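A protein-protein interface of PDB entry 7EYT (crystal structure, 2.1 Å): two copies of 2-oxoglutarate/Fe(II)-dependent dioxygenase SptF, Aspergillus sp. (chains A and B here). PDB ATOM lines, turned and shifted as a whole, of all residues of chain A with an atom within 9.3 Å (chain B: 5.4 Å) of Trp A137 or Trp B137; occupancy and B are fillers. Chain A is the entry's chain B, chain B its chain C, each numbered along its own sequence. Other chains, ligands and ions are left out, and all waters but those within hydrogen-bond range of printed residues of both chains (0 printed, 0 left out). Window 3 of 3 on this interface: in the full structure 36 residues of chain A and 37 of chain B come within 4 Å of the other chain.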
ATOM      1  N   MET A  98     -32.281   8.532  -0.622  1.00  0.00           N
ATOM      2  CA  MET A  98     -31.167   8.911   0.237  1.00  0.00           C
ATOM      3  C   MET A  98     -29.813   8.632  -0.407  1.00  0.00           C
ATOM      4  O   MET A  98     -28.870   9.405  -0.217  1.00  0.00           O
ATOM      5  CB  MET A  98     -31.278   8.187   1.581  1.00  0.00           C
ATOM      6  CG  MET A  98     -30.062   8.315   2.483  1.00  0.00           C
ATOM      7  SD  MET A  98     -30.335   7.518   4.077  1.00  0.00           S
ATOM      8  CE  MET A  98     -32.067   7.897   4.328  1.00  0.00           C
ATOM      9  N   PHE A  99     -29.703   7.549  -1.176  1.00  0.00           N
ATOM     10  CA  PHE A  99     -28.448   7.181  -1.818  1.00  0.00           C
ATOM     11  C   PHE A  99     -28.419   7.475  -3.312  1.00  0.00           C
ATOM     12  O   PHE A  99     -27.329   7.649  -3.869  1.00  0.00           O
ATOM     13  CB  PHE A  99     -28.161   5.689  -1.605  1.00  0.00           C
ATOM     14  CG  PHE A  99     -28.148   5.269  -0.161  1.00  0.00           C
ATOM     15  CD1 PHE A  99     -27.371   5.944   0.766  1.00  0.00           C
ATOM     16  CD2 PHE A  99     -28.905   4.191   0.265  1.00  0.00           C
ATOM     17  CE1 PHE A  99     -27.355   5.556   2.093  1.00  0.00           C
ATOM     18  CE2 PHE A  99     -28.893   3.796   1.590  1.00  0.00           C
ATOM     19  CZ  PHE A  99     -28.117   4.479   2.506  1.00  0.00           C
ATOM     20  N   THR A 102     -26.680  10.847  -5.016  1.00  0.00           N
ATOM     21  CA  THR A 102     -25.257  10.969  -4.730  1.00  0.00           C
ATOM     22  C   THR A 102     -24.469   9.728  -5.136  1.00  0.00           C
ATOM     23  O   THR A 102     -23.380   9.847  -5.707  1.00  0.00           O
ATOM     24  CB  THR A 102     -25.046  11.252  -3.240  1.00  0.00           C
ATOM     25  OG1 THR A 102     -25.732  12.458  -2.881  1.00  0.00           O
ATOM     26  CG2 THR A 102     -23.564  11.404  -2.925  1.00  0.00           C
ATOM     27  N   TYR A 103     -25.003   8.536  -4.864  1.00  0.00           N
ATOM     28  CA  TYR A 103     -24.270   7.297  -5.070  1.00  0.00           C
ATOM     29  C   TYR A 103     -24.803   6.433  -6.203  1.00  0.00           C
ATOM     30  O   TYR A 103     -24.080   5.547  -6.669  1.00  0.00           O
ATOM     31  CB  TYR A 103     -24.274   6.460  -3.785  1.00  0.00           C
ATOM     32  CG  TYR A 103     -23.451   7.054  -2.671  1.00  0.00           C
ATOM     33  CD1 TYR A 103     -22.073   6.889  -2.640  1.00  0.00           C
ATOM     34  CD2 TYR A 103     -24.051   7.780  -1.651  1.00  0.00           C
ATOM     35  CE1 TYR A 103     -21.316   7.428  -1.622  1.00  0.00           C
ATOM     36  CE2 TYR A 103     -23.301   8.321  -0.630  1.00  0.00           C
ATOM     37  CZ  TYR A 103     -21.935   8.140  -0.620  1.00  0.00           C
ATOM     38  OH  TYR A 103     -21.184   8.677   0.394  1.00  0.00           O
ATOM     39  N   HIS A 129     -22.856   4.123  11.788  1.00  0.00           N
ATOM     40  CA  HIS A 129     -21.787   4.322  10.819  1.00  0.00           C
ATOM     41  C   HIS A 129     -20.418   4.470  11.476  1.00  0.00           C
ATOM     42  O   HIS A 129     -19.484   4.971  10.839  1.00  0.00           O
ATOM     43  CB  HIS A 129     -22.093   5.533   9.930  1.00  0.00           C
ATOM     44  CG  HIS A 129     -22.114   6.848  10.653  1.00  0.00           C
ATOM     45  ND1 HIS A 129     -22.652   7.988  10.096  1.00  0.00           N
ATOM     46  CD2 HIS A 129     -21.659   7.208  11.877  1.00  0.00           C
ATOM     47  CE1 HIS A 129     -22.527   8.993  10.943  1.00  0.00           C
ATOM     48  NE2 HIS A 129     -21.928   8.547  12.032  1.00  0.00           N
ATOM     49  N   TYR A 132     -17.401   2.762   9.660  1.00  0.00           N
ATOM     50  CA  TYR A 132     -16.893   3.318   8.412  1.00  0.00           C
ATOM     51  C   TYR A 132     -15.800   4.324   8.749  1.00  0.00           C
ATOM     52  O   TYR A 132     -16.072   5.342   9.394  1.00  0.00           O
ATOM     53  CB  TYR A 132     -17.998   4.006   7.610  1.00  0.00           C
ATOM     54  CG  TYR A 132     -19.101   3.104   7.114  1.00  0.00           C
ATOM     55  CD1 TYR A 132     -20.199   2.820   7.912  1.00  0.00           C
ATOM     56  CD2 TYR A 132     -19.061   2.559   5.837  1.00  0.00           C
ATOM     57  CE1 TYR A 132     -21.219   2.008   7.464  1.00  0.00           C
ATOM     58  CE2 TYR A 132     -20.077   1.742   5.378  1.00  0.00           C
ATOM     59  CZ  TYR A 132     -21.155   1.472   6.198  1.00  0.00           C
ATOM     60  OH  TYR A 132     -22.174   0.661   5.757  1.00  0.00           O
ATOM     61  N   GLN A 133     -14.568   4.040   8.324  1.00  0.00           N
ATOM     62  CA  GLN A 133     -13.490   4.999   8.535  1.00  0.00           C
ATOM     63  C   GLN A 133     -13.798   6.335   7.875  1.00  0.00           C
ATOM     64  O   GLN A 133     -13.338   7.383   8.344  1.00  0.00           O
ATOM     65  CB  GLN A 133     -12.171   4.441   8.000  1.00  0.00           C
ATOM     66  N   ILE A 134     -14.589   6.319   6.803  1.00  0.00           N
ATOM     67  CA  ILE A 134     -14.889   7.511   6.022  1.00  0.00           C
ATOM     68  C   ILE A 134     -15.955   8.347   6.717  1.00  0.00           C
ATOM     69  O   ILE A 134     -16.317   9.426   6.235  1.00  0.00           O
ATOM     70  CB  ILE A 134     -15.333   7.128   4.598  1.00  0.00           C
ATOM     71  CG1 ILE A 134     -16.402   6.035   4.652  1.00  0.00           C
ATOM     72  CG2 ILE A 134     -14.141   6.672   3.774  1.00  0.00           C
ATOM     73  CD1 ILE A 134     -17.068   5.768   3.323  1.00  0.00           C
ATOM     74  N   SER A 135     -16.476   7.855   7.846  1.00  0.00           N
ATOM     75  CA  SER A 135     -17.433   8.647   8.608  1.00  0.00           C
ATOM     76  C   SER A 135     -16.793   9.891   9.206  1.00  0.00           C
ATOM     77  O   SER A 135     -17.506  10.849   9.526  1.00  0.00           O
ATOM     78  CB  SER A 135     -18.071   7.805   9.717  1.00  0.00           C
ATOM     79  OG  SER A 135     -17.140   7.514  10.747  1.00  0.00           O
ATOM     80  N   LYS A 136     -15.470   9.903   9.351  1.00  0.00           N
ATOM     81  CA  LYS A 136     -14.749  11.057   9.868  1.00  0.00           C
ATOM     82  C   LYS A 136     -14.448  12.098   8.799  1.00  0.00           C
ATOM     83  O   LYS A 136     -13.885  13.149   9.124  1.00  0.00           O
ATOM     84  CB  LYS A 136     -13.453  10.599  10.540  1.00  0.00           C
ATOM     85  CG  LYS A 136     -13.687   9.782  11.802  1.00  0.00           C
ATOM     86  CD  LYS A 136     -13.022   8.420  11.718  1.00  0.00           C
ATOM     87  CE  LYS A 136     -11.559   8.493  12.115  1.00  0.00           C
ATOM     88  NZ  LYS A 136     -11.142   7.294  12.895  1.00  0.00           N
ATOM     89  N   TRP A 137     -14.797  11.833   7.539  1.00  0.00           N
ATOM     90  CA  TRP A 137     -14.757  12.850   6.497  1.00  0.00           C
ATOM     91  C   TRP A 137     -16.136  13.391   6.153  1.00  0.00           C
ATOM     92  O   TRP A 137     -16.232  14.443   5.511  1.00  0.00           O
ATOM     93  CB  TRP A 137     -14.117  12.301   5.213  1.00  0.00           C
ATOM     94  CG  TRP A 137     -12.861  11.499   5.406  1.00  0.00           C
ATOM     95  CD1 TRP A 137     -12.011  11.537   6.473  1.00  0.00           C
ATOM     96  CD2 TRP A 137     -12.303  10.555   4.483  1.00  0.00           C
ATOM     97  NE1 TRP A 137     -10.967  10.664   6.278  1.00  0.00           N
ATOM     98  CE2 TRP A 137     -11.122  10.050   5.063  1.00  0.00           C
ATOM     99  CE3 TRP A 137     -12.692  10.083   3.225  1.00  0.00           C
ATOM    100  CZ2 TRP A 137     -10.328   9.098   4.427  1.00  0.00           C
ATOM    101  CZ3 TRP A 137     -11.901   9.139   2.596  1.00  0.00           C
ATOM    102  CH2 TRP A 137     -10.733   8.657   3.198  1.00  0.00           C
ATOM    103  N   ARG A 138     -17.194  12.700   6.565  1.00  0.00           N
ATOM    104  CA  ARG A 138     -18.553  13.084   6.218  1.00  0.00           C
ATOM    105  C   ARG A 138     -19.021  14.255   7.072  1.00  0.00           C
ATOM    106  O   ARG A 138     -18.705  14.343   8.262  1.00  0.00           O
ATOM    107  CB  ARG A 138     -19.496  11.893   6.398  1.00  0.00           C
ATOM    108  CG  ARG A 138     -20.921  12.134   5.931  1.00  0.00           C
ATOM    109  CD  ARG A 138     -21.823  10.967   6.307  1.00  0.00           C
ATOM    110  NE  ARG A 138     -23.172  11.402   6.648  1.00  0.00           N
ATOM    111  CZ  ARG A 138     -23.547  11.807   7.854  1.00  0.00           C
ATOM    112  NH1 ARG A 138     -22.695  11.851   8.864  1.00  0.00           N
ATOM    113  NH2 ARG A 138     -24.810  12.176   8.050  1.00  0.00           N
ATOM    114  N   ARG A 139     -19.784  15.163   6.448  1.00  0.00           N
ATOM    115  CA  ARG A 139     -20.441  16.278   7.111  1.00  0.00           C
ATOM    116  C   ARG A 139     -21.868  15.895   7.493  1.00  0.00           C
ATOM    117  O   ARG A 139     -22.488  15.056   6.832  1.00  0.00           O
ATOM    118  CB  ARG A 139     -20.463  17.502   6.198  1.00  0.00           C
ATOM    119  N   PRO A 140     -22.410  16.483   8.564  1.00  0.00           N
ATOM    120  CA  PRO A 140     -23.774  16.121   8.985  1.00  0.00           C
ATOM    121  C   PRO A 140     -24.837  16.393   7.933  1.00  0.00           C
ATOM    122  O   PRO A 140     -25.893  15.751   7.967  1.00  0.00           O
ATOM    123  CB  PRO A 140     -23.995  16.982  10.237  1.00  0.00           C
ATOM    124  CG  PRO A 140     -22.619  17.279  10.738  1.00  0.00           C
ATOM    125  CD  PRO A 140     -21.763  17.403   9.514  1.00  0.00           C
ATOM    126  N   THR A 141     -24.595  17.314   7.003  1.00  0.00           N
ATOM    127  CA  THR A 141     -25.539  17.586   5.927  1.00  0.00           C
ATOM    128  C   THR A 141     -25.371  16.651   4.737  1.00  0.00           C
ATOM    129  O   THR A 141     -26.257  16.607   3.875  1.00  0.00           O
ATOM    130  CB  THR A 141     -25.406  19.041   5.457  1.00  0.00           C
ATOM    131  OG1 THR A 141     -24.021  19.364   5.279  1.00  0.00           O
ATOM    132  CG2 THR A 141     -26.017  19.988   6.479  1.00  0.00           C
ATOM    133  N   ASP A 142     -24.265  15.913   4.667  1.00  0.00           N
ATOM    134  CA  ASP A 142     -24.069  14.935   3.612  1.00  0.00           C
ATOM    135  C   ASP A 142     -25.059  13.782   3.770  1.00  0.00           C
ATOM    136  O   ASP A 142     -25.612  13.569   4.852  1.00  0.00           O
ATOM    137  CB  ASP A 142     -22.638  14.404   3.643  1.00  0.00           C
ATOM    138  CG  ASP A 142     -21.647  15.358   3.005  1.00  0.00           C
ATOM    139  OD1 ASP A 142     -22.080  16.396   2.462  1.00  0.00           O
ATOM    140  OD2 ASP A 142     -20.433  15.064   3.045  1.00  0.00           O
ATOM    141  N   PRO A 143     -25.309  13.026   2.699  1.00  0.00           N
ATOM    142  CA  PRO A 143     -26.168  11.844   2.828  1.00  0.00           C
ATOM    143  C   PRO A 143     -25.541  10.804   3.744  1.00  0.00           C
ATOM    144  O   PRO A 143     -24.318  10.715   3.877  1.00  0.00           O
ATOM    145  CB  PRO A 143     -26.285  11.327   1.388  1.00  0.00           C
ATOM    146  CG  PRO A 143     -25.117  11.924   0.667  1.00  0.00           C
ATOM    147  CD  PRO A 143     -24.900  13.259   1.303  1.00  0.00           C
ATOM    148  N   ASP A 144     -26.399  10.013   4.381  1.00  0.00           N
ATOM    149  CA  ASP A 144     -25.935   9.014   5.332  1.00  0.00           C
ATOM    150  C   ASP A 144     -25.164   7.904   4.626  1.00  0.00           C
ATOM    151  O   ASP A 144     -25.367   7.629   3.441  1.00  0.00           O
ATOM    152  CB  ASP A 144     -27.116   8.421   6.101  1.00  0.00           C
ATOM    153  CG  ASP A 144     -27.603   9.331   7.212  1.00  0.00           C
ATOM    154  OD1 ASP A 144     -26.998   9.309   8.304  1.00  0.00           O
ATOM    155  OD2 ASP A 144     -28.588  10.067   6.995  1.00  0.00           O
ATOM    156  N   LEU A 145     -24.263   7.265   5.375  1.00  0.00           N
ATOM    157  CA  LEU A 145     -23.493   6.148   4.843  1.00  0.00           C
ATOM    158  C   LEU A 145     -24.251   4.830   4.904  1.00  0.00           C
ATOM    159  O   LEU A 145     -23.879   3.885   4.202  1.00  0.00           O
ATOM    160  CB  LEU A 145     -22.170   6.008   5.599  1.00  0.00           C
ATOM    161  CG  LEU A 145     -21.231   7.214   5.596  1.00  0.00           C
ATOM    162  CD1 LEU A 145     -20.170   7.058   6.672  1.00  0.00           C
ATOM    163  CD2 LEU A 145     -20.589   7.392   4.228  1.00  0.00           C
ATOM    164  N   THR A 146     -25.293   4.743   5.729  1.00  0.00           N
ATOM    165  CA  THR A 146     -26.083   3.526   5.855  1.00  0.00           C
ATOM    166  C   THR A 146     -27.386   3.871   6.557  1.00  0.00           C
ATOM    167  O   THR A 146     -27.488   4.884   7.254  1.00  0.00           O
ATOM    168  CB  THR A 146     -25.326   2.432   6.623  1.00  0.00           C
ATOM    169  OG1 THR A 146     -26.174   1.291   6.799  1.00  0.00           O
ATOM    170  CG2 THR A 146     -24.882   2.943   7.985  1.00  0.00           C
ATOM    171  N   ASN A 174     -19.206  15.924  13.912  1.00  0.00           N
ATOM    172  CA  ASN A 174     -18.424  14.724  14.172  1.00  0.00           C
ATOM    173  C   ASN A 174     -17.462  14.970  15.328  1.00  0.00           C
ATOM    174  O   ASN A 174     -16.765  15.988  15.366  1.00  0.00           O
ATOM    175  CB  ASN A 174     -17.661  14.307  12.916  1.00  0.00           C
ATOM    176  CG  ASN A 174     -18.519  14.373  11.669  1.00  0.00           C
ATOM    177  OD1 ASN A 174     -19.046  15.430  11.320  1.00  0.00           O
ATOM    178  ND2 ASN A 174     -18.671  13.240  10.995  1.00  0.00           N
ATOM    179  N   PRO A 223     -24.644   2.578   0.250  1.00  0.00           N
ATOM    180  CA  PRO A 223     -24.253   2.791  -1.149  1.00  0.00           C
ATOM    181  C   PRO A 223     -23.508   1.602  -1.745  1.00  0.00           C
ATOM    182  O   PRO A 223     -22.784   0.882  -1.052  1.00  0.00           O
ATOM    183  CB  PRO A 223     -23.357   4.028  -1.079  1.00  0.00           C
ATOM    184  CG  PRO A 223     -23.901   4.796   0.067  1.00  0.00           C
ATOM    185  CD  PRO A 223     -24.394   3.783   1.069  1.00  0.00           C
ATOM    186  N   PHE A 226     -19.707   0.704  -1.255  1.00  0.00           N
ATOM    187  CA  PHE A 226     -19.226   0.280   0.052  1.00  0.00           C
ATOM    188  C   PHE A 226     -19.422  -1.222   0.212  1.00  0.00           C
ATOM    189  O   PHE A 226     -20.448  -1.772  -0.201  1.00  0.00           O
ATOM    190  CB  PHE A 226     -19.951   1.023   1.180  1.00  0.00           C
ATOM    191  CG  PHE A 226     -19.828   2.520   1.104  1.00  0.00           C
ATOM    192  CD1 PHE A 226     -18.749   3.114   0.464  1.00  0.00           C
ATOM    193  CD2 PHE A 226     -20.790   3.334   1.678  1.00  0.00           C
ATOM    194  CE1 PHE A 226     -18.639   4.489   0.393  1.00  0.00           C
ATOM    195  CE2 PHE A 226     -20.684   4.711   1.612  1.00  0.00           C
ATOM    196  CZ  PHE A 226     -19.608   5.289   0.967  1.00  0.00           C
ATOM    197  N   TYR B 103      -7.521   1.305   7.204  1.00  0.00           N
ATOM    198  CA  TYR B 103      -8.655   0.485   6.807  1.00  0.00           C
ATOM    199  C   TYR B 103      -8.537  -0.969   7.232  1.00  0.00           C
ATOM    200  O   TYR B 103      -9.528  -1.703   7.139  1.00  0.00           O
ATOM    201  CB  TYR B 103      -8.837   0.533   5.284  1.00  0.00           C
ATOM    202  CG  TYR B 103      -9.092   1.914   4.733  1.00  0.00           C
ATOM    203  CD1 TYR B 103     -10.383   2.418   4.646  1.00  0.00           C
ATOM    204  CD2 TYR B 103      -8.045   2.710   4.293  1.00  0.00           C
ATOM    205  CE1 TYR B 103     -10.623   3.677   4.138  1.00  0.00           C
ATOM    206  CE2 TYR B 103      -8.274   3.971   3.782  1.00  0.00           C
ATOM    207  CZ  TYR B 103      -9.565   4.450   3.709  1.00  0.00           C
ATOM    208  OH  TYR B 103      -9.798   5.706   3.201  1.00  0.00           O
ATOM    209  N   GLN B 133     -17.121   8.595  -5.364  1.00  0.00           N
ATOM    210  CA  GLN B 133     -17.835   9.770  -4.875  1.00  0.00           C
ATOM    211  C   GLN B 133     -17.162  10.350  -3.638  1.00  0.00           C
ATOM    212  O   GLN B 133     -17.151  11.572  -3.449  1.00  0.00           O
ATOM    213  CB  GLN B 133     -19.292   9.412  -4.573  1.00  0.00           C
ATOM    214  CG  GLN B 133     -20.062  10.482  -3.811  1.00  0.00           C
ATOM    215  CD  GLN B 133     -20.451  11.661  -4.682  1.00  0.00           C
ATOM    216  OE1 GLN B 133     -19.957  12.774  -4.498  1.00  0.00           O
ATOM    217  NE2 GLN B 133     -21.344  11.423  -5.636  1.00  0.00           N
ATOM    218  N   ILE B 134     -16.576   9.491  -2.796  1.00  0.00           N
ATOM    219  CA  ILE B 134     -15.952   9.950  -1.557  1.00  0.00           C
ATOM    220  C   ILE B 134     -14.609  10.626  -1.776  1.00  0.00           C
ATOM    221  O   ILE B 134     -14.025  11.136  -0.812  1.00  0.00           O
ATOM    222  CB  ILE B 134     -15.770   8.781  -0.571  1.00  0.00           C
ATOM    223  CG1 ILE B 134     -15.052   7.616  -1.252  1.00  0.00           C
ATOM    224  CG2 ILE B 134     -17.117   8.336  -0.019  1.00  0.00           C
ATOM    225  CD1 ILE B 134     -14.582   6.551  -0.291  1.00  0.00           C
ATOM    226  N   SER B 135     -14.095  10.643  -3.009  1.00  0.00           N
ATOM    227  CA  SER B 135     -12.877  11.395  -3.280  1.00  0.00           C
ATOM    228  C   SER B 135     -13.091  12.895  -3.132  1.00  0.00           C
ATOM    229  O   SER B 135     -12.123  13.629  -2.906  1.00  0.00           O
ATOM    230  CB  SER B 135     -12.349  11.073  -4.681  1.00  0.00           C
ATOM    231  OG  SER B 135     -13.146  11.674  -5.686  1.00  0.00           O
ATOM    232  N   LYS B 136     -14.336  13.364  -3.252  1.00  0.00           N
ATOM    233  CA  LYS B 136     -14.631  14.761  -2.955  1.00  0.00           C
ATOM    234  C   LYS B 136     -14.541  15.043  -1.461  1.00  0.00           C
ATOM    235  O   LYS B 136     -14.271  16.180  -1.060  1.00  0.00           O
ATOM    236  CB  LYS B 136     -16.018  15.128  -3.483  1.00  0.00           C
ATOM    237  CG  LYS B 136     -16.193  14.916  -4.979  1.00  0.00           C
ATOM    238  CD  LYS B 136     -15.983  16.210  -5.760  1.00  0.00           C
ATOM    239  CE  LYS B 136     -16.492  17.425  -4.994  1.00  0.00           C
ATOM    240  NZ  LYS B 136     -16.578  18.635  -5.858  1.00  0.00           N
ATOM    241  N   TRP B 137     -14.766  14.026  -0.626  1.00  0.00           N
ATOM    242  CA  TRP B 137     -14.640  14.180   0.817  1.00  0.00           C
ATOM    243  C   TRP B 137     -13.197  14.105   1.292  1.00  0.00           C
ATOM    244  O   TRP B 137     -12.886  14.615   2.374  1.00  0.00           O
ATOM    245  CB  TRP B 137     -15.442  13.101   1.547  1.00  0.00           C
ATOM    246  CG  TRP B 137     -16.915  13.106   1.284  1.00  0.00           C
ATOM    247  CD1 TRP B 137     -17.624  14.023   0.566  1.00  0.00           C
ATOM    248  CD2 TRP B 137     -17.863  12.143   1.756  1.00  0.00           C
ATOM    249  NE1 TRP B 137     -18.957  13.686   0.556  1.00  0.00           N
ATOM    250  CE2 TRP B 137     -19.129  12.536   1.280  1.00  0.00           C
ATOM    251  CE3 TRP B 137     -17.763  10.984   2.532  1.00  0.00           C
ATOM    252  CZ2 TRP B 137     -20.285  11.811   1.556  1.00  0.00           C
ATOM    253  CZ3 TRP B 137     -18.911  10.267   2.803  1.00  0.00           C
ATOM    254  CH2 TRP B 137     -20.156  10.685   2.321  1.00  0.00           C
ATOM    255  N   ARG B 138     -12.318  13.481   0.514  1.00  0.00           N
ATOM    256  CA  ARG B 138     -10.978  13.137   0.962  1.00  0.00           C
ATOM    257  C   ARG B 138     -10.024  14.309   0.771  1.00  0.00           C
ATOM    258  O   ARG B 138      -9.926  14.869  -0.325  1.00  0.00           O
ATOM    259  CB  ARG B 138     -10.470  11.912   0.199  1.00  0.00           C
ATOM    260  CG  ARG B 138      -9.007  11.589   0.424  1.00  0.00           C
ATOM    261  CD  ARG B 138      -8.513  10.586  -0.604  1.00  0.00           C
ATOM    262  NE  ARG B 138      -7.088  10.312  -0.460  1.00  0.00           N
ATOM    263  CZ  ARG B 138      -6.131  10.974  -1.094  1.00  0.00           C
ATOM    264  NH1 ARG B 138      -6.410  11.959  -1.933  1.00  0.00           N
ATOM    265  NH2 ARG B 138      -4.862  10.640  -0.881  1.00  0.00           N
ATOM    266  N   ARG B 139      -9.322  14.673   1.843  1.00  0.00           N
ATOM    267  CA  ARG B 139      -8.267  15.668   1.754  1.00  0.00           C
ATOM    268  C   ARG B 139      -6.980  15.020   1.244  1.00  0.00           C
ATOM    269  O   ARG B 139      -6.757  13.824   1.449  1.00  0.00           O
ATOM    270  CB  ARG B 139      -8.026  16.312   3.117  1.00  0.00           C
ATOM    271  CG  ARG B 139      -9.295  16.619   3.901  1.00  0.00           C
ATOM    272  CD  ARG B 139     -10.075  17.775   3.291  1.00  0.00           C
ATOM    273  NE  ARG B 139      -9.221  18.695   2.546  1.00  0.00           N
ATOM    274  CZ  ARG B 139      -8.622  19.756   3.069  1.00  0.00           C
ATOM    275  NH1 ARG B 139      -8.757  20.065   4.349  1.00  0.00           N
ATOM    276  NH2 ARG B 139      -7.869  20.526   2.289  1.00  0.00           N
ATOM    277  N   ASP B 142      -4.914  12.575   3.336  1.00  0.00           N
ATOM    278  CA  ASP B 142      -5.431  11.269   3.704  1.00  0.00           C
ATOM    279  C   ASP B 142      -4.752  10.170   2.889  1.00  0.00           C
ATOM    280  O   ASP B 142      -4.127  10.441   1.862  1.00  0.00           O
ATOM    281  CB  ASP B 142      -6.942  11.219   3.485  1.00  0.00           C
ATOM    282  CG  ASP B 142      -7.663  12.390   4.119  1.00  0.00           C
ATOM    283  OD1 ASP B 142      -7.149  12.941   5.115  1.00  0.00           O
ATOM    284  OD2 ASP B 142      -8.745  12.760   3.619  1.00  0.00           O
ATOM    285  N   PRO B 143      -4.846   8.919   3.340  1.00  0.00           N
ATOM    286  CA  PRO B 143      -4.386   7.804   2.506  1.00  0.00           C
ATOM    287  C   PRO B 143      -5.189   7.717   1.216  1.00  0.00           C
ATOM    288  O   PRO B 143      -6.313   8.212   1.113  1.00  0.00           O
ATOM    289  CB  PRO B 143      -4.613   6.570   3.391  1.00  0.00           C
ATOM    290  CG  PRO B 143      -5.549   7.025   4.470  1.00  0.00           C
ATOM    291  CD  PRO B 143      -5.243   8.469   4.685  1.00  0.00           C
ATOM    292  N   LEU B 145      -7.319   6.267  -2.006  1.00  0.00           N
ATOM    293  CA  LEU B 145      -8.468   5.386  -2.158  1.00  0.00           C
ATOM    294  C   LEU B 145      -8.138   4.127  -2.944  1.00  0.00           C
ATOM    295  O   LEU B 145      -8.824   3.113  -2.782  1.00  0.00           O
ATOM    296  CB  LEU B 145      -9.613   6.128  -2.848  1.00  0.00           C
ATOM    297  CG  LEU B 145     -10.136   7.377  -2.138  1.00  0.00           C
ATOM    298  CD1 LEU B 145     -11.162   8.082  -3.004  1.00  0.00           C
ATOM    299  CD2 LEU B 145     -10.728   7.021  -0.786  1.00  0.00           C
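Of the 11 printed residues of chain B, 5 touch a printed residue of chain A. Hydrophobic or aromatic side chains of chain A within 4 Å of the printed part of chain B: Tyr A103, Trp A137 and Leu A145. Among the printed residues, 10 pairs touch across the chains. Among the printed residues, no Asp or Glu carboxylate lies within 4 Å of a Lys or Arg side-chain nitrogen of the other chain.
Tyr A103 touches Gln B133. OH of Tyr A103 touches CH2 of Trp B137, at 3.0 Å. CH2 of Trp A137 touches OH of Tyr B103, 3.1 Å away. CB of Trp A137 touches O of Trp B137, at 3.9 Å. Arg B138 touches Trp A137 (CB to CZ3, 3.9 Å). Trp A137 touches Asp B142 (CE2 to OD2, 3.9 Å). Trp B137 touches Arg A138 (CH2 to CG, 3.96 Å). CZ3 of Trp B137 touches CD2 of Leu A145, at 3.6 Å.
Tyr A103 touches Gln B133, but with the chains exchanged Gln A133 does not touch Tyr B103 (4.2 Å). Trp A137 touches Arg B138, and with the chains exchanged Arg A138 touches Trp B137. Trp A137 touches Asp B142, and with the chains exchanged Asp A142 touches Trp B137. Leu A145 touches Trp B137, but with the chains exchanged Trp A137 does not touch Leu B145 (4.2 Å). Positions printed for both chains: 103, 133, 134, 135, 136, 137, 138, 139, 142, 143 and 145. Of the 10 pairs that touch across the chains among the printed residues, 7 have their exchanged pair printed and touching as well.
The backbone carbonyl oxygen (O) of Asp B142 sits at hydrogen-bond distance from the guanidinium group (NH2) of Arg B138 (2.8 Å). The guanidinium group (NH2) of Arg A138 is in salt-bridge range of the side-chain carboxylate (OD1) of Asp A144. The side-chain carboxylate of Asp A142 is in hydrogen-bond range of the backbone NH of Arg A139 (3.5 Å). The guanidinium group of Arg A138 sits at hydrogen-bond distance from the backbone carbonyl oxygen of Pro A143, at 3.1 Å. The guanidinium group (NE) of Arg B138 is in hydrogen-bond range of the backbone carbonyl oxygen (O) of Pro B143. The side-chain carboxylate of Asp B142 is in hydrogen-bond range of the backbone NH of Arg B139.
NE1 of Trp B137 is in hydrogen-bond range of OD2 of Asp A142, at 3.2 Å. NE2 of Gln B133 is in hydrogen-bond range of O of Thr A102.
Of chain B, only Tyr B103 (3.1 Å), Trp B137 (3.9 Å), Arg B138 (3.9 Å) and Asp B142 (3.9 Å) come within 4 Å of Trp A137. Of chain A, only Tyr A103 (3.0 Å), Trp A137 (3.9 Å), Arg A138 (3.96 Å), Asp A142 (3.2 Å) and Leu A145 (3.6 Å) come within 4 Å of Trp B137. Printed residues of chain A within 4 Å of Arg B138: Trp A137. Printed residues of chain B within 4 Å of Leu A145: Trp B137. Printed residues of chain B within 4 Å of Arg A138: Trp B137. Printed residues of chain B within 4 Å of Tyr A103: Gln B133 and Trp B137. Printed residues of chain A within 4 Å of Tyr B103: Trp A137 (3.1 Å). Ile B134 touches none of the printed residues of chain A. Thr A146 touches none of the printed residues of chain B. The nearest residue of chain B that does not touch Trp A137 is Leu B145 (4.2 Å). The nearest printed residue of chain B that does not touch Thr A102 is Trp B137 (5.6 Å).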
